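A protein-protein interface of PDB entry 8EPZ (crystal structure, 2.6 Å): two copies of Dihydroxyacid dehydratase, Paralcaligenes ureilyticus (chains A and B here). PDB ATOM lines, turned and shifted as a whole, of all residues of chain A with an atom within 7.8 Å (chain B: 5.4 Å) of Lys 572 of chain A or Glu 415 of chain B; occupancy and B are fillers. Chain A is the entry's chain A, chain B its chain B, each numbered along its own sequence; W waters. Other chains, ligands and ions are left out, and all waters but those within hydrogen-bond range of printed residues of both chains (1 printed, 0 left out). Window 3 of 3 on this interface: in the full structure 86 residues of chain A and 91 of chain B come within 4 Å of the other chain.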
ATOM      1  N   TRP A  14      20.656  -2.166  16.861  1.00  0.00           N
ATOM      2  CA  TRP A  14      20.326  -3.166  15.852  1.00  0.00           C
ATOM      3  C   TRP A  14      19.952  -2.512  14.525  1.00  0.00           C
ATOM      4  O   TRP A  14      20.617  -2.718  13.506  1.00  0.00           O
ATOM      5  CB  TRP A  14      19.144  -4.036  16.309  1.00  0.00           C
ATOM      6  CG  TRP A  14      19.389  -5.011  17.420  1.00  0.00           C
ATOM      7  CD1 TRP A  14      19.494  -6.367  17.309  1.00  0.00           C
ATOM      8  CD2 TRP A  14      19.497  -4.715  18.817  1.00  0.00           C
ATOM      9  NE1 TRP A  14      19.680  -6.931  18.546  1.00  0.00           N
ATOM     10  CE2 TRP A  14      19.685  -5.938  19.489  1.00  0.00           C
ATOM     11  CE3 TRP A  14      19.462  -3.535  19.564  1.00  0.00           C
ATOM     12  CZ2 TRP A  14      19.841  -6.015  20.872  1.00  0.00           C
ATOM     13  CZ3 TRP A  14      19.617  -3.613  20.936  1.00  0.00           C
ATOM     14  CH2 TRP A  14      19.805  -4.843  21.575  1.00  0.00           C
ATOM     15  N   ARG A  17      22.008   0.525  12.224  1.00  0.00           N
ATOM     16  CA  ARG A  17      23.406   0.230  11.946  1.00  0.00           C
ATOM     17  C   ARG A  17      23.649   0.233  10.443  1.00  0.00           C
ATOM     18  O   ARG A  17      22.926  -0.426   9.688  1.00  0.00           O
ATOM     19  CB  ARG A  17      23.797  -1.118  12.551  1.00  0.00           C
ATOM     20  CG  ARG A  17      23.884  -1.104  14.066  1.00  0.00           C
ATOM     21  CD  ARG A  17      25.310  -0.876  14.536  1.00  0.00           C
ATOM     22  NE  ARG A  17      26.164  -2.023  14.235  1.00  0.00           N
ATOM     23  CZ  ARG A  17      26.459  -2.982  15.105  1.00  0.00           C
ATOM     24  NH1 ARG A  17      25.976  -2.932  16.340  1.00  0.00           N
ATOM     25  NH2 ARG A  17      27.243  -3.989  14.743  1.00  0.00           N
ATOM     26  N   ASP A  21      26.191  -5.958   9.956  1.00  0.00           N
ATOM     27  CA  ASP A  21      25.243  -6.409  10.966  1.00  0.00           C
ATOM     28  C   ASP A  21      23.897  -5.710  10.814  1.00  0.00           C
ATOM     29  O   ASP A  21      22.845  -6.330  11.007  1.00  0.00           O
ATOM     30  CB  ASP A  21      25.832  -6.176  12.356  1.00  0.00           C
ATOM     31  CG  ASP A  21      26.976  -7.123  12.665  1.00  0.00           C
ATOM     32  OD1 ASP A  21      26.873  -7.879  13.654  1.00  0.00           O
ATOM     33  OD2 ASP A  21      27.964  -7.136  11.901  1.00  0.00           O
ATOM     34  N   TYR A  25      20.072  -7.475  11.049  1.00  0.00           N
ATOM     35  CA  TYR A  25      19.035  -7.106  12.003  1.00  0.00           C
ATOM     36  C   TYR A  25      17.764  -6.582  11.349  1.00  0.00           C
ATOM     37  O   TYR A  25      16.739  -6.482  12.029  1.00  0.00           O
ATOM     38  CB  TYR A  25      19.576  -6.056  12.977  1.00  0.00           C
ATOM     39  CG  TYR A  25      20.807  -6.507  13.727  1.00  0.00           C
ATOM     40  CD1 TYR A  25      21.939  -5.709  13.782  1.00  0.00           C
ATOM     41  CD2 TYR A  25      20.832  -7.724  14.391  1.00  0.00           C
ATOM     42  CE1 TYR A  25      23.066  -6.117  14.460  1.00  0.00           C
ATOM     43  CE2 TYR A  25      21.955  -8.141  15.080  1.00  0.00           C
ATOM     44  CZ  TYR A  25      23.070  -7.332  15.111  1.00  0.00           C
ATOM     45  OH  TYR A  25      24.194  -7.734  15.792  1.00  0.00           O
ATOM     46  N   GLY A 113      18.099  -9.135  25.318  1.00  0.00           N
ATOM     47  CA  GLY A 113      18.634  -9.652  24.072  1.00  0.00           C
ATOM     48  C   GLY A 113      17.941  -9.170  22.818  1.00  0.00           C
ATOM     49  O   GLY A 113      18.490  -9.337  21.726  1.00  0.00           O
ATOM     50  N   GLY A 569      21.709  -2.379  29.027  1.00  0.00           N
ATOM     51  CA  GLY A 569      22.712  -1.839  28.135  1.00  0.00           C
ATOM     52  C   GLY A 569      22.777  -2.614  26.830  1.00  0.00           C
ATOM     53  O   GLY A 569      22.102  -3.624  26.624  1.00  0.00           O
ATOM     54  N   ILE A 570      23.618  -2.120  25.924  1.00  0.00           N
ATOM     55  CA  ILE A 570      23.759  -2.728  24.600  1.00  0.00           C
ATOM     56  C   ILE A 570      24.640  -3.967  24.718  1.00  0.00           C
ATOM     57  O   ILE A 570      25.788  -3.868  25.177  1.00  0.00           O
ATOM     58  CB  ILE A 570      24.330  -1.731  23.576  1.00  0.00           C
ATOM     59  CG1 ILE A 570      23.209  -0.939  22.906  1.00  0.00           C
ATOM     60  CG2 ILE A 570      25.128  -2.449  22.497  1.00  0.00           C
ATOM     61  CD1 ILE A 570      22.387  -0.107  23.839  1.00  0.00           C
ATOM     62  N   PRO A 571      24.146  -5.145  24.350  1.00  0.00           N
ATOM     63  CA  PRO A 571      25.000  -6.334  24.322  1.00  0.00           C
ATOM     64  C   PRO A 571      25.792  -6.403  23.023  1.00  0.00           C
ATOM     65  O   PRO A 571      25.552  -5.662  22.068  1.00  0.00           O
ATOM     66  CB  PRO A 571      24.005  -7.500  24.429  1.00  0.00           C
ATOM     67  CG  PRO A 571      22.665  -6.868  24.738  1.00  0.00           C
ATOM     68  CD  PRO A 571      22.731  -5.492  24.161  1.00  0.00           C
ATOM     69  N   LYS A 572      26.755  -7.322  23.005  1.00  0.00           N
ATOM     70  CA  LYS A 572      27.628  -7.472  21.853  1.00  0.00           C
ATOM     71  C   LYS A 572      26.854  -7.998  20.648  1.00  0.00           C
ATOM     72  O   LYS A 572      25.765  -8.566  20.772  1.00  0.00           O
ATOM     73  CB  LYS A 572      28.784  -8.412  22.188  1.00  0.00           C
ATOM     74  CG  LYS A 572      29.661  -7.920  23.326  1.00  0.00           C
ATOM     75  CD  LYS A 572      30.495  -9.046  23.903  1.00  0.00           C
ATOM     76  CE  LYS A 572      31.264  -9.773  22.817  1.00  0.00           C
ATOM     77  NZ  LYS A 572      32.167  -8.853  22.067  1.00  0.00           N
ATOM     78  N   ASP A 573      27.429  -7.791  19.464  1.00  0.00           N
ATOM     79  CA  ASP A 573      26.834  -8.318  18.244  1.00  0.00           C
ATOM     80  C   ASP A 573      26.795  -9.840  18.289  1.00  0.00           C
ATOM     81  O   ASP A 573      27.593 -10.485  18.973  1.00  0.00           O
ATOM     82  CB  ASP A 573      27.619  -7.856  17.017  1.00  0.00           C
ATOM     83  CG  ASP A 573      27.659  -6.350  16.883  1.00  0.00           C
ATOM     84  OD1 ASP A 573      28.647  -5.735  17.338  1.00  0.00           O
ATOM     85  OD2 ASP A 573      26.700  -5.779  16.323  1.00  0.00           O
ATOM     86  N   ASN A 574      25.853 -10.416  17.547  1.00  0.00           N
ATOM     87  CA  ASN A 574      25.679 -11.861  17.515  1.00  0.00           C
ATOM     88  C   ASN A 574      26.349 -12.520  16.317  1.00  0.00           C
ATOM     89  O   ASN A 574      26.222 -13.737  16.148  1.00  0.00           O
ATOM     90  CB  ASN A 574      24.187 -12.217  17.549  1.00  0.00           C
ATOM     91  CG  ASN A 574      23.355 -11.383  16.589  1.00  0.00           C
ATOM     92  OD1 ASN A 574      23.840 -10.934  15.550  1.00  0.00           O
ATOM     93  ND2 ASN A 574      22.091 -11.174  16.935  1.00  0.00           N
ATOM     94  N   HIS A 575      27.062 -11.758  15.494  1.00  0.00           N
ATOM     95  CA  HIS A 575      27.793 -12.326  14.367  1.00  0.00           C
ATOM     96  C   HIS A 575      29.160 -11.664  14.211  1.00  0.00           C
ATOM     97  O   HIS A 575      29.304 -10.456  14.406  1.00  0.00           O
ATOM     98  CB  HIS A 575      26.989 -12.185  13.072  1.00  0.00           C
ATOM     99  CG  HIS A 575      25.803 -13.096  12.992  1.00  0.00           C
ATOM    100  ND1 HIS A 575      24.650 -12.890  13.720  1.00  0.00           N
ATOM    101  CD2 HIS A 575      25.592 -14.221  12.267  1.00  0.00           C
ATOM    102  CE1 HIS A 575      23.781 -13.846  13.447  1.00  0.00           C
ATOM    103  NE2 HIS A 575      24.326 -14.665  12.568  1.00  0.00           N
ATOM    104  N   ARG B  93      20.884 -11.059  21.321  1.00  0.00           N
ATOM    105  CA  ARG B  93      22.251 -10.651  21.580  1.00  0.00           C
ATOM    106  C   ARG B  93      22.543 -10.883  23.056  1.00  0.00           C
ATOM    107  O   ARG B  93      21.648 -10.697  23.895  1.00  0.00           O
ATOM    108  CB  ARG B  93      22.479  -9.177  21.231  1.00  0.00           C
ATOM    109  CG  ARG B  93      22.626  -8.879  19.752  1.00  0.00           C
ATOM    110  CD  ARG B  93      22.734  -7.378  19.558  1.00  0.00           C
ATOM    111  NE  ARG B  93      23.488  -6.992  18.372  1.00  0.00           N
ATOM    112  CZ  ARG B  93      23.880  -5.746  18.126  1.00  0.00           C
ATOM    113  NH1 ARG B  93      23.588  -4.779  18.985  1.00  0.00           N
ATOM    114  NH2 ARG B  93      24.569  -5.463  17.030  1.00  0.00           N
ATOM    115  N   PRO B  94      23.781 -11.270  23.419  1.00  0.00           N
ATOM    116  CA  PRO B  94      24.994 -11.473  22.613  1.00  0.00           C
ATOM    117  C   PRO B  94      24.874 -12.544  21.530  1.00  0.00           C
ATOM    118  O   PRO B  94      25.540 -12.432  20.504  1.00  0.00           O
ATOM    119  CB  PRO B  94      26.036 -11.900  23.655  1.00  0.00           C
ATOM    120  CG  PRO B  94      25.536 -11.352  24.937  1.00  0.00           C
ATOM    121  CD  PRO B  94      24.049 -11.462  24.854  1.00  0.00           C
ATOM    122  N   THR B  95      24.044 -13.560  21.762  1.00  0.00           N
ATOM    123  CA  THR B  95      23.779 -14.602  20.776  1.00  0.00           C
ATOM    124  C   THR B  95      22.593 -15.429  21.249  1.00  0.00           C
ATOM    125  O   THR B  95      22.319 -15.516  22.450  1.00  0.00           O
ATOM    126  CB  THR B  95      25.000 -15.506  20.551  1.00  0.00           C
ATOM    127  OG1 THR B  95      24.689 -16.495  19.559  1.00  0.00           O
ATOM    128  CG2 THR B  95      25.398 -16.199  21.842  1.00  0.00           C
ATOM    129  N   ASN B 413      39.950 -11.311  21.731  1.00  0.00           N
ATOM    130  CA  ASN B 413      38.521 -11.524  21.914  1.00  0.00           C
ATOM    131  C   ASN B 413      37.809 -10.979  20.681  1.00  0.00           C
ATOM    132  O   ASN B 413      38.436 -10.714  19.650  1.00  0.00           O
ATOM    133  CB  ASN B 413      38.023 -10.888  23.218  1.00  0.00           C
ATOM    134  CG  ASN B 413      38.349  -9.410  23.320  1.00  0.00           C
ATOM    135  OD1 ASN B 413      38.409  -8.699  22.319  1.00  0.00           O
ATOM    136  ND2 ASN B 413      38.554  -8.937  24.544  1.00  0.00           N
ATOM    137  N   SER B 414      36.493 -10.811  20.785  1.00  0.00           N
ATOM    138  CA  SER B 414      35.735 -10.284  19.658  1.00  0.00           C
ATOM    139  C   SER B 414      35.859  -8.768  19.559  1.00  0.00           C
ATOM    140  O   SER B 414      35.918  -8.222  18.451  1.00  0.00           O
ATOM    141  CB  SER B 414      34.270 -10.695  19.777  1.00  0.00           C
ATOM    142  OG  SER B 414      33.736 -10.259  21.010  1.00  0.00           O
ATOM    143  N   GLU B 415      35.894  -8.073  20.701  1.00  0.00           N
ATOM    144  CA  GLU B 415      36.137  -6.633  20.681  1.00  0.00           C
ATOM    145  C   GLU B 415      37.484  -6.327  20.043  1.00  0.00           C
ATOM    146  O   GLU B 415      37.577  -5.520  19.111  1.00  0.00           O
ATOM    147  CB  GLU B 415      36.077  -6.055  22.097  1.00  0.00           C
ATOM    148  CG  GLU B 415      34.914  -6.527  22.949  1.00  0.00           C
ATOM    149  CD  GLU B 415      35.231  -7.796  23.715  1.00  0.00           C
ATOM    150  OE1 GLU B 415      35.342  -8.865  23.080  1.00  0.00           O
ATOM    151  OE2 GLU B 415      35.383  -7.722  24.953  1.00  0.00           O
ATOM    152  N   HIS B 416      38.543  -6.980  20.535  1.00  0.00           N
ATOM    153  CA  HIS B 416      39.874  -6.790  19.973  1.00  0.00           C
ATOM    154  C   HIS B 416      39.930  -7.202  18.510  1.00  0.00           C
ATOM    155  O   HIS B 416      40.682  -6.612  17.728  1.00  0.00           O
ATOM    156  CB  HIS B 416      40.894  -7.582  20.794  1.00  0.00           C
ATOM    157  CG  HIS B 416      42.310  -7.402  20.346  1.00  0.00           C
ATOM    158  ND1 HIS B 416      42.984  -8.356  19.611  1.00  0.00           N
ATOM    159  CD2 HIS B 416      43.186  -6.389  20.541  1.00  0.00           C
ATOM    160  CE1 HIS B 416      44.211  -7.933  19.369  1.00  0.00           C
ATOM    161  NE2 HIS B 416      44.359  -6.743  19.921  1.00  0.00           N
ATOM    162  N   MET B 417      39.141  -8.207  18.119  1.00  0.00           N
ATOM    163  CA  MET B 417      39.089  -8.599  16.715  1.00  0.00           C
ATOM    164  C   MET B 417      38.454  -7.512  15.857  1.00  0.00           C
ATOM    165  O   MET B 417      38.854  -7.324  14.703  1.00  0.00           O
ATOM    166  CB  MET B 417      38.326  -9.916  16.567  1.00  0.00           C
ATOM    167  CG  MET B 417      38.413 -10.542  15.182  1.00  0.00           C
ATOM    168  SD  MET B 417      36.970 -10.195  14.160  1.00  0.00           S
ATOM    169  CE  MET B 417      35.660 -10.811  15.214  1.00  0.00           C
ATOM    170  N   HIS B 418      37.473  -6.787  16.397  1.00  0.00           N
ATOM    171  CA  HIS B 418      36.854  -5.705  15.642  1.00  0.00           C
ATOM    172  C   HIS B 418      37.692  -4.433  15.683  1.00  0.00           C
ATOM    173  O   HIS B 418      37.661  -3.646  14.729  1.00  0.00           O
ATOM    174  CB  HIS B 418      35.443  -5.430  16.168  1.00  0.00           C
ATOM    175  CG  HIS B 418      34.462  -6.523  15.869  1.00  0.00           C
ATOM    176  ND1 HIS B 418      34.179  -6.941  14.586  1.00  0.00           N
ATOM    177  CD2 HIS B 418      33.691  -7.278  16.687  1.00  0.00           C
ATOM    178  CE1 HIS B 418      33.281  -7.909  14.627  1.00  0.00           C
ATOM    179  NE2 HIS B 418      32.968  -8.134  15.890  1.00  0.00           N
ATOM    180  N   GLU B 419      38.447  -4.215  16.763  1.00  0.00           N
ATOM    181  CA  GLU B 419      39.342  -3.066  16.846  1.00  0.00           C
ATOM    182  C   GLU B 419      40.566  -3.203  15.953  1.00  0.00           C
ATOM    183  O   GLU B 419      41.263  -2.207  15.732  1.00  0.00           O
ATOM    184  CB  GLU B 419      39.815  -2.862  18.289  1.00  0.00           C
ATOM    185  CG  GLU B 419      38.724  -2.541  19.291  1.00  0.00           C
ATOM    186  CD  GLU B 419      39.259  -2.428  20.709  1.00  0.00           C
ATOM    187  OE1 GLU B 419      39.867  -3.403  21.199  1.00  0.00           O
ATOM    188  OE2 GLU B 419      39.084  -1.359  21.329  1.00  0.00           O
ATOM    189  N   ARG B 420      40.842  -4.398  15.433  1.00  0.00           N
ATOM    190  CA  ARG B 420      42.148  -4.685  14.856  1.00  0.00           C
ATOM    191  C   ARG B 420      42.059  -5.210  13.427  1.00  0.00           C
ATOM    192  O   ARG B 420      42.999  -5.041  12.643  1.00  0.00           O
ATOM    193  CB  ARG B 420      42.885  -5.685  15.753  1.00  0.00           C
ATOM    194  CG  ARG B 420      44.230  -6.135  15.239  1.00  0.00           C
ATOM    195  CD  ARG B 420      44.974  -6.983  16.256  1.00  0.00           C
ATOM    196  NE  ARG B 420      46.180  -7.571  15.684  1.00  0.00           N
ATOM    197  CZ  ARG B 420      47.172  -8.100  16.394  1.00  0.00           C
ATOM    198  NH1 ARG B 420      47.110  -8.113  17.717  1.00  0.00           N
ATOM    199  NH2 ARG B 420      48.229  -8.612  15.776  1.00  0.00           N
ATOM    200  N   TYR B 444      32.020 -15.567  25.066  1.00  0.00           N
ATOM    201  CA  TYR B 444      31.376 -14.411  24.455  1.00  0.00           C
ATOM    202  C   TYR B 444      30.617 -13.566  25.463  1.00  0.00           C
ATOM    203  O   TYR B 444      30.821 -12.344  25.471  1.00  0.00           O
ATOM    204  CB  TYR B 444      30.490 -14.883  23.303  1.00  0.00           C
ATOM    205  CG  TYR B 444      30.392 -13.865  22.202  1.00  0.00           C
ATOM    206  CD1 TYR B 444      31.434 -13.688  21.307  1.00  0.00           C
ATOM    207  CD2 TYR B 444      29.267 -13.066  22.066  1.00  0.00           C
ATOM    208  CE1 TYR B 444      31.361 -12.751  20.299  1.00  0.00           C
ATOM    209  CE2 TYR B 444      29.178 -12.127  21.061  1.00  0.00           C
ATOM    210  CZ  TYR B 444      30.229 -11.970  20.177  1.00  0.00           C
ATOM    211  OH  TYR B 444      30.156 -11.035  19.168  1.00  0.00           O
HETATM  212  O   HOH W   1      31.170 -10.005  16.933  1.00  0.00           O
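The side-chain carboxylate (OD1) of Asp 21 of chain A is in hydrogen-bond range of the side-chain hydroxyl (OH) of Tyr 25 of chain A (3.4 Å). OD1 of Asn 574 of chain A is in hydrogen-bond range of OH of Tyr 25 of chain A, 3.2 Å away. The side-chain hydroxyl of Ser 414 of chain B is in hydrogen-bond range of the side-chain carboxylate of Glu 415 of chain B (3.0 Å). A ring nitrogen (ND1) of His 575 of chain A sits at hydrogen-bond distance from the side-chain amide oxygen (OD1) of Asn 574 of chain A (2.8 Å). OH of Tyr 25 of chain A lies within hydrogen-bond range of OD2 of Asp 573 of chain A, at 3.2 Å. The guanidinium group of Arg 17 of chain A lies within salt-bridge range of the side-chain carboxylate of Asp 573 of chain A.
Among the printed residues, pairs that only touch across the chains: Trp 14 of chain A with Arg 93 of chain B (3.2 Å), Pro 571 of chain A with Arg 93 of chain B (3.8 Å), Pro 571 of chain A with Pro 94 of chain B (3.9 Å), Lys 572 of chain A with Arg 93 of chain B (3.3 Å), Lys 572 of chain A with Pro 94 of chain B (3.5 Å), Lys 572 of chain A with Tyr 444 of chain B (3.6 Å), Asn 574 of chain A with Arg 93 of chain B (3.7 Å) and Asn 574 of chain A with Pro 94 of chain B (3.0 Å).
Water W1 lies within hydrogen-bond range of OH of Tyr 444 of chain B (2.7 Å), NE2 of His 418 of chain B (2.8 Å) and O of His 575 of chain A (3.2 Å).
The side-chain carboxylate of Asp 573 of chain A is in salt-bridge range of the guanidinium group of Arg 93 of chain B (3.998 Å). O of Pro 94 of chain B lies close to O of Asp 573 of chain A (3.2 Å). OH of Tyr 444 of chain B is in hydrogen-bond range of O of Asp 573 of chain A (2.6 Å). OH of Tyr 25 of chain A is in hydrogen-bond range of NH2 of Arg 93 of chain B. N of Arg 93 of chain B lies within hydrogen-bond range of O of Gly 113 of chain A, at 3.0 Å. The guanidinium group (NH1) of Arg 17 of chain A sits close to the guanidinium group (NH2) of Arg 93 of chain B, 3.0 Å away. OG of Ser 414 of chain B lies close to NZ of Lys 572 of chain A (2.4 Å). The side-chain amino group of Lys 572 of chain A lies within salt-bridge range of the side-chain carboxylate of Glu 415 of chain B, at 3.3 Å.
Of chain B, only Arg 93, Pro 94, Ser 414, Glu 415 and Tyr 444 come within 4 Å of Lys 572 of chain A. Printed residues of chain A within 4 Å of Glu 415 of chain B: Lys 572. Printed residues of chain A within 4 Å of Ser 414 of chain B: Lys 572 (2.4 Å). Printed residues of chain A within 4 Å of Tyr 444 of chain B: Lys 572 and Asp 573. Printed residues of chain B within 4 Å of Arg 17 of chain A: Arg 93. Of the printed residues of chain A, Arg 93 of chain B touches Trp 14 (3.2 Å), Arg 17 (3.0 Å), Tyr 25 (2.6 Å), Gly 113 (3.0 Å), Pro 571 (3.8 Å), Lys 572 (3.3 Å), Asp 573 (2.3 Å) and Asn 574 (3.7 Å). Of the printed residues of chain B, Trp 14 of chain A touches Arg 93. The nearest printed residue of chain B that does not touch Gly 113 of chain A is Pro 94 of chain B (5.4 Å).
No position is printed for both chains.
Of the 12 printed residues of chain B, 5 touch a printed residue of chain A. Printed residues of chain B that touch a printed residue of chain A: Arg 93, Pro 94, Ser 414, Glu 415 and Tyr 444. Hydrophobic or aromatic side chains of chain B that line the printed part of chain A: Pro 94 and Tyr 444. Hydrophobic or aromatic side chains of chain A that line the printed part of chain B: Trp 14, Tyr 25 and Pro 571.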
